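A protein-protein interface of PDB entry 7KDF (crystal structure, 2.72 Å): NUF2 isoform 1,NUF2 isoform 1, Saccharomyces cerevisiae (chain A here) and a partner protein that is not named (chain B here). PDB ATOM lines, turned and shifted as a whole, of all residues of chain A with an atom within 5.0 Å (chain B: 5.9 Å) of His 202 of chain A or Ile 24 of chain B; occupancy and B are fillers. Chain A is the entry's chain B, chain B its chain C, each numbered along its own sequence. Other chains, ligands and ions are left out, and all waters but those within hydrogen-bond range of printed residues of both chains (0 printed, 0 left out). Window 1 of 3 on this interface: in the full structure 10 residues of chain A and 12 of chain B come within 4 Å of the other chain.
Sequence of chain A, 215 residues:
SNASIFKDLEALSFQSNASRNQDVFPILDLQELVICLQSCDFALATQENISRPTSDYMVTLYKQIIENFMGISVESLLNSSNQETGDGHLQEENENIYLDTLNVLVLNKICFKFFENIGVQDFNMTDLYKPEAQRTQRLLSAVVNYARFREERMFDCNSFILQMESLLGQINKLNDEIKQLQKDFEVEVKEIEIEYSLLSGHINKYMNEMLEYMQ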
ATOM      1  N   SER A 197       9.035 -10.353  -5.722  1.00  0.00           N
ATOM      2  CA  SER A 197       7.658 -10.595  -5.302  1.00  0.00           C
ATOM      3  C   SER A 197       6.946  -9.290  -4.978  1.00  0.00           C
ATOM      4  O   SER A 197       5.766  -9.122  -5.307  1.00  0.00           O
ATOM      5  CB  SER A 197       7.627 -11.540  -4.104  1.00  0.00           C
ATOM      6  OG  SER A 197       7.802 -12.881  -4.521  1.00  0.00           O
ATOM      7  N   LEU A 198       7.647  -8.353  -4.336  1.00  0.00           N
ATOM      8  CA  LEU A 198       7.078  -7.032  -4.099  1.00  0.00           C
ATOM      9  C   LEU A 198       6.708  -6.359  -5.414  1.00  0.00           C
ATOM     10  O   LEU A 198       5.604  -5.821  -5.565  1.00  0.00           O
ATOM     11  CB  LEU A 198       8.068  -6.169  -3.316  1.00  0.00           C
ATOM     12  CG  LEU A 198       8.334  -6.610  -1.877  1.00  0.00           C
ATOM     13  CD1 LEU A 198       9.283  -5.648  -1.169  1.00  0.00           C
ATOM     14  CD2 LEU A 198       7.016  -6.736  -1.120  1.00  0.00           C
ATOM     15  N   LEU A 199       7.617  -6.399  -6.388  1.00  0.00           N
ATOM     16  CA  LEU A 199       7.347  -5.772  -7.677  1.00  0.00           C
ATOM     17  C   LEU A 199       6.220  -6.484  -8.414  1.00  0.00           C
ATOM     18  O   LEU A 199       5.406  -5.838  -9.081  1.00  0.00           O
ATOM     19  CB  LEU A 199       8.621  -5.747  -8.520  1.00  0.00           C
ATOM     20  CG  LEU A 199       8.453  -5.291  -9.967  1.00  0.00           C
ATOM     21  CD1 LEU A 199       8.096  -3.822 -10.000  1.00  0.00           C
ATOM     22  CD2 LEU A 199       9.729  -5.538 -10.738  1.00  0.00           C
ATOM     23  N   SER A 200       6.159  -7.815  -8.313  1.00  0.00           N
ATOM     24  CA  SER A 200       5.081  -8.554  -8.963  1.00  0.00           C
ATOM     25  C   SER A 200       3.726  -8.172  -8.382  1.00  0.00           C
ATOM     26  O   SER A 200       2.754  -7.986  -9.124  1.00  0.00           O
ATOM     27  CB  SER A 200       5.310 -10.058  -8.829  1.00  0.00           C
ATOM     28  OG  SER A 200       4.231 -10.782  -9.397  1.00  0.00           O
ATOM     29  N   GLY A 201       3.643  -8.057  -7.057  1.00  0.00           N
ATOM     30  CA  GLY A 201       2.406  -7.604  -6.443  1.00  0.00           C
ATOM     31  C   GLY A 201       2.073  -6.173  -6.812  1.00  0.00           C
ATOM     32  O   GLY A 201       0.903  -5.825  -6.994  1.00  0.00           O
ATOM     33  N   HIS A 202       3.100  -5.327  -6.933  1.00  0.00           N
ATOM     34  CA  HIS A 202       2.891  -3.933  -7.313  1.00  0.00           C
ATOM     35  C   HIS A 202       2.281  -3.817  -8.706  1.00  0.00           C
ATOM     36  O   HIS A 202       1.367  -3.014  -8.924  1.00  0.00           O
ATOM     37  CB  HIS A 202       4.220  -3.180  -7.240  1.00  0.00           C
ATOM     38  CG  HIS A 202       4.079  -1.692  -7.196  1.00  0.00           C
ATOM     39  ND1 HIS A 202       3.866  -0.997  -6.024  1.00  0.00           N
ATOM     40  CD2 HIS A 202       4.144  -0.762  -8.178  1.00  0.00           C
ATOM     41  CE1 HIS A 202       3.795   0.295  -6.289  1.00  0.00           C
ATOM     42  NE2 HIS A 202       3.962   0.465  -7.588  1.00  0.00           N
ATOM     43  N   ILE A 203       2.776  -4.605  -9.664  1.00  0.00           N
ATOM     44  CA  ILE A 203       2.254  -4.542 -11.025  1.00  0.00           C
ATOM     45  C   ILE A 203       0.831  -5.088 -11.089  1.00  0.00           C
ATOM     46  O   ILE A 203      -0.031  -4.524 -11.778  1.00  0.00           O
ATOM     47  CB  ILE A 203       3.197  -5.288 -11.987  1.00  0.00           C
ATOM     48  CG1 ILE A 203       4.584  -4.640 -11.985  1.00  0.00           C
ATOM     49  CG2 ILE A 203       2.617  -5.330 -13.395  1.00  0.00           C
ATOM     50  CD1 ILE A 203       5.581  -5.321 -12.899  1.00  0.00           C
ATOM     51  N   ASN A 204       0.568  -6.205 -10.394  1.00  0.00           N
ATOM     52  CA  ASN A 204      -0.796  -6.723 -10.298  1.00  0.00           C
ATOM     53  C   ASN A 204      -1.728  -5.755  -9.588  1.00  0.00           C
ATOM     54  O   ASN A 204      -2.878  -5.588 -10.004  1.00  0.00           O
ATOM     55  CB  ASN A 204      -0.801  -8.091  -9.615  1.00  0.00           C
ATOM     56  CG  ASN A 204      -0.375  -9.210 -10.546  1.00  0.00           C
ATOM     57  OD1 ASN A 204       0.716  -9.767 -10.433  1.00  0.00           O
ATOM     58  ND2 ASN A 204      -1.315  -9.635 -11.392  1.00  0.00           N
ATOM     59  N   LYS A 205      -1.266  -5.124  -8.508  1.00  0.00           N
ATOM     60  CA  LYS A 205      -2.089  -4.111  -7.856  1.00  0.00           C
ATOM     61  C   LYS A 205      -2.424  -2.986  -8.832  1.00  0.00           C
ATOM     62  O   LYS A 205      -3.589  -2.593  -8.967  1.00  0.00           O
ATOM     63  CB  LYS A 205      -1.368  -3.585  -6.613  1.00  0.00           C
ATOM     64  CG  LYS A 205      -2.146  -2.553  -5.802  1.00  0.00           C
ATOM     65  CD  LYS A 205      -1.325  -2.142  -4.586  1.00  0.00           C
ATOM     66  CE  LYS A 205      -2.017  -1.035  -3.797  1.00  0.00           C
ATOM     67  NZ  LYS A 205      -1.144  -0.691  -2.633  1.00  0.00           N
ATOM     68  N   TYR A 206      -1.415  -2.510  -9.571  1.00  0.00           N
ATOM     69  CA  TYR A 206      -1.595  -1.454 -10.568  1.00  0.00           C
ATOM     70  C   TYR A 206      -2.660  -1.807 -11.607  1.00  0.00           C
ATOM     71  O   TYR A 206      -3.552  -1.003 -11.899  1.00  0.00           O
ATOM     72  CB  TYR A 206      -0.249  -1.193 -11.244  1.00  0.00           C
ATOM     73  CG  TYR A 206      -0.277  -0.263 -12.429  1.00  0.00           C
ATOM     74  CD1 TYR A 206      -0.461   1.101 -12.258  1.00  0.00           C
ATOM     75  CD2 TYR A 206      -0.088  -0.745 -13.717  1.00  0.00           C
ATOM     76  CE1 TYR A 206      -0.473   1.960 -13.335  1.00  0.00           C
ATOM     77  CE2 TYR A 206      -0.100   0.106 -14.802  1.00  0.00           C
ATOM     78  CZ  TYR A 206      -0.294   1.459 -14.606  1.00  0.00           C
ATOM     79  OH  TYR A 206      -0.310   2.315 -15.684  1.00  0.00           O
ATOM     80  N   GLU A 209      -6.345  -1.787 -10.121  1.00  0.00           N
ATOM     81  CA  GLU A 209      -6.939  -0.461  -9.987  1.00  0.00           C
ATOM     82  C   GLU A 209      -7.291   0.133 -11.349  1.00  0.00           C
ATOM     83  O   GLU A 209      -8.344   0.763 -11.503  1.00  0.00           O
ATOM     84  CB  GLU A 209      -5.997   0.464  -9.220  1.00  0.00           C
ATOM     85  CG  GLU A 209      -5.576  -0.072  -7.862  1.00  0.00           C
ATOM     86  CD  GLU A 209      -5.272   1.030  -6.861  1.00  0.00           C
ATOM     87  OE1 GLU A 209      -5.650   2.194  -7.122  1.00  0.00           O
ATOM     88  OE2 GLU A 209      -4.654   0.728  -5.815  1.00  0.00           O
ATOM     89  N   ARG B  19      10.156  -0.396  -8.718  1.00  0.00           N
ATOM     90  CA  ARG B  19       8.871  -0.439  -8.028  1.00  0.00           C
ATOM     91  C   ARG B  19       8.519   0.917  -7.429  1.00  0.00           C
ATOM     92  O   ARG B  19       7.357   1.340  -7.468  1.00  0.00           O
ATOM     93  CB  ARG B  19       8.898  -1.510  -6.937  1.00  0.00           C
ATOM     94  CG  ARG B  19       7.671  -1.519  -6.044  1.00  0.00           C
ATOM     95  CD  ARG B  19       7.668  -2.715  -5.100  1.00  0.00           C
ATOM     96  NE  ARG B  19       8.887  -2.791  -4.299  1.00  0.00           N
ATOM     97  CZ  ARG B  19       9.037  -2.222  -3.108  1.00  0.00           C
ATOM     98  NH1 ARG B  19       8.040  -1.530  -2.570  1.00  0.00           N
ATOM     99  NH2 ARG B  19      10.184  -2.343  -2.453  1.00  0.00           N
ATOM    100  N   GLU B  20       9.509   1.610  -6.864  1.00  0.00           N
ATOM    101  CA  GLU B  20       9.242   2.899  -6.236  1.00  0.00           C
ATOM    102  C   GLU B  20       9.018   4.006  -7.260  1.00  0.00           C
ATOM    103  O   GLU B  20       8.434   5.039  -6.919  1.00  0.00           O
ATOM    104  CB  GLU B  20      10.388   3.251  -5.288  1.00  0.00           C
ATOM    105  CG  GLU B  20      10.484   2.289  -4.110  1.00  0.00           C
ATOM    106  CD  GLU B  20      11.500   2.714  -3.071  1.00  0.00           C
ATOM    107  OE1 GLU B  20      12.463   3.428  -3.428  1.00  0.00           O
ATOM    108  OE2 GLU B  20      11.336   2.324  -1.894  1.00  0.00           O
ATOM    109  N   PHE B  22       7.270   3.203  -9.967  1.00  0.00           N
ATOM    110  CA  PHE B  22       6.063   2.701 -10.616  1.00  0.00           C
ATOM    111  C   PHE B  22       4.865   3.373  -9.952  1.00  0.00           C
ATOM    112  O   PHE B  22       4.159   2.791  -9.124  1.00  0.00           O
ATOM    113  CB  PHE B  22       6.007   1.183 -10.507  1.00  0.00           C
ATOM    114  CG  PHE B  22       5.229   0.518 -11.598  1.00  0.00           C
ATOM    115  CD1 PHE B  22       5.881  -0.099 -12.647  1.00  0.00           C
ATOM    116  CD2 PHE B  22       3.845   0.487 -11.562  1.00  0.00           C
ATOM    117  CE1 PHE B  22       5.171  -0.726 -13.647  1.00  0.00           C
ATOM    118  CE2 PHE B  22       3.129  -0.138 -12.560  1.00  0.00           C
ATOM    119  CZ  PHE B  22       3.794  -0.746 -13.604  1.00  0.00           C
ATOM    120  N   ASP B  23       4.645   4.633 -10.324  1.00  0.00           N
ATOM    121  CA  ASP B  23       3.605   5.451  -9.708  1.00  0.00           C
ATOM    122  C   ASP B  23       2.235   4.954 -10.149  1.00  0.00           C
ATOM    123  O   ASP B  23       1.856   5.105 -11.315  1.00  0.00           O
ATOM    124  CB  ASP B  23       3.805   6.914 -10.088  1.00  0.00           C
ATOM    125  CG  ASP B  23       3.076   7.865  -9.160  1.00  0.00           C
ATOM    126  OD1 ASP B  23       2.059   7.460  -8.555  1.00  0.00           O
ATOM    127  OD2 ASP B  23       3.525   9.024  -9.037  1.00  0.00           O
ATOM    128  N   ILE B  24       1.481   4.367  -9.220  1.00  0.00           N
ATOM    129  CA  ILE B  24       0.159   3.853  -9.560  1.00  0.00           C
ATOM    130  C   ILE B  24      -0.878   4.972  -9.552  1.00  0.00           C
ATOM    131  O   ILE B  24      -1.696   5.085 -10.473  1.00  0.00           O
ATOM    132  CB  ILE B  24      -0.234   2.712  -8.604  1.00  0.00           C
ATOM    133  CG1 ILE B  24       0.527   1.436  -8.956  1.00  0.00           C
ATOM    134  CG2 ILE B  24      -1.734   2.461  -8.656  1.00  0.00           C
ATOM    135  CD1 ILE B  24       0.595   0.434  -7.827  1.00  0.00           C
ATOM    136  N   GLN B  25      -0.859   5.816  -8.516  1.00  0.00           N
ATOM    137  CA  GLN B  25      -1.905   6.824  -8.364  1.00  0.00           C
ATOM    138  C   GLN B  25      -1.917   7.797  -9.535  1.00  0.00           C
ATOM    139  O   GLN B  25      -2.989   8.199 -10.005  1.00  0.00           O
ATOM    140  CB  GLN B  25      -1.728   7.574  -7.043  1.00  0.00           C
ATOM    141  CG  GLN B  25      -3.025   8.155  -6.490  1.00  0.00           C
ATOM    142  CD  GLN B  25      -4.105   7.101  -6.289  1.00  0.00           C
ATOM    143  OE1 GLN B  25      -3.812   5.926  -6.050  1.00  0.00           O
ATOM    144  NE2 GLN B  25      -5.364   7.517  -6.407  1.00  0.00           N
ATOM    145  N   GLN B  26      -0.736   8.189 -10.017  1.00  0.00           N
ATOM    146  CA  GLN B  26      -0.650   9.091 -11.160  1.00  0.00           C
ATOM    147  C   GLN B  26      -1.466   8.573 -12.341  1.00  0.00           C
ATOM    148  O   GLN B  26      -2.298   9.296 -12.902  1.00  0.00           O
ATOM    149  CB  GLN B  26       0.813   9.280 -11.551  1.00  0.00           C
ATOM    150  CG  GLN B  26       1.126  10.569 -12.280  1.00  0.00           C
ATOM    151  CD  GLN B  26       2.584  10.643 -12.700  1.00  0.00           C
ATOM    152  OE1 GLN B  26       3.167   9.655 -13.159  1.00  0.00           O
ATOM    153  NE2 GLN B  26       3.184  11.816 -12.545  1.00  0.00           N
ATOM    154  N   ASP B  27      -1.262   7.307 -12.713  1.00  0.00           N
ATOM    155  CA  ASP B  27      -1.982   6.754 -13.857  1.00  0.00           C
ATOM    156  C   ASP B  27      -3.463   6.549 -13.546  1.00  0.00           C
ATOM    157  O   ASP B  27      -4.318   6.737 -14.424  1.00  0.00           O
ATOM    158  CB  ASP B  27      -1.329   5.447 -14.299  1.00  0.00           C
ATOM    159  CG  ASP B  27       0.108   5.642 -14.767  1.00  0.00           C
ATOM    160  OD1 ASP B  27       0.585   6.796 -14.754  1.00  0.00           O
ATOM    161  OD2 ASP B  27       0.760   4.646 -15.150  1.00  0.00           O
ATOM    162  N   VAL B  28      -3.794   6.164 -12.311  1.00  0.00           N
ATOM    163  CA  VAL B  28      -5.203   6.024 -11.948  1.00  0.00           C
ATOM    164  C   VAL B  28      -5.896   7.378 -12.001  1.00  0.00           C
ATOM    165  O   VAL B  28      -7.005   7.508 -12.537  1.00  0.00           O
ATOM    166  CB  VAL B  28      -5.342   5.370 -10.561  1.00  0.00           C
ATOM    167  CG1 VAL B  28      -6.756   5.565 -10.027  1.00  0.00           C
ATOM    168  CG2 VAL B  28      -5.002   3.895 -10.636  1.00  0.00           C
ATOM    169  N   ASP B  29      -5.245   8.411 -11.458  1.00  0.00           N
ATOM    170  CA  ASP B  29      -5.799   9.759 -11.528  1.00  0.00           C
ATOM    171  C   ASP B  29      -6.001  10.188 -12.972  1.00  0.00           C
ATOM    172  O   ASP B  29      -7.037  10.771 -13.315  1.00  0.00           O
ATOM    173  CB  ASP B  29      -4.878  10.741 -10.809  1.00  0.00           C
ATOM    174  CG  ASP B  29      -5.091  10.750  -9.312  1.00  0.00           C
ATOM    175  OD1 ASP B  29      -6.042  10.094  -8.840  1.00  0.00           O
ATOM    176  OD2 ASP B  29      -4.306  11.418  -8.610  1.00  0.00           O
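A ring nitrogen (NE2) of His 202 of chain A sits at hydrogen-bond distance from the backbone carbonyl oxygen (O) of Phe 22 of chain B. OD2 of Asp 27 of chain B lies within hydrogen-bond range of OH of Tyr 206 of chain A (2.6 Å).
Leu 198 of chain A touches Arg 19 of chain B (CB to NE, 3.6 Å). Arg 19 of chain B touches Leu 199 of chain A (CD to N, 3.9 Å). His 202 of chain A touches Arg 19 of chain B. NE2 of His 202 of chain A touches CD1 of Ile 24 of chain B (3.4 Å). Tyr 206 of chain A touches Phe 22 of chain B. CD1 of Tyr 206 of chain A touches CG1 of Ile 24 of chain B, at 3.5 Å. Glu 209 of chain A touches Val 28 of chain B.
Printed residues of chain B within 4 Å of Leu 198 of chain A: Arg 19. Of chain B, only Arg 19, Phe 22 and Ile 24 come within 4 Å of His 202 of chain A. Of the printed residues of chain A, Phe 22 of chain B touches His 202 and Tyr 206. Ile 24 of chain B touches two residues of chain A. The nearest printed residue of chain A that does not touch Phe 22 of chain B is Ile 203 of chain A (4.3 Å).
Printed residues of chain B that touch a printed residue of chain A: Arg 19, Phe 22, Ile 24, Asp 27 and Val 28. Hydrophobic or aromatic side chains of chain B that line the printed part of chain A: Phe 22, Ile 24 and Val 28. Printed residues of chain A that touch a printed residue of chain B: Leu 198, Leu 199, His 202, Tyr 206 and Glu 209. Hydrophobic or aromatic side chains of chain A within 4 Å of the printed part of chain B: Leu 198, Leu 199, His 202 and Tyr 206. Along chain A the printed residues that touch a printed residue of chain B span positions 198 to 209. Among the printed residues, no Asp or Glu carboxylate lies within 4 Å of a Lys or Arg side-chain nitrogen of the other chain.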
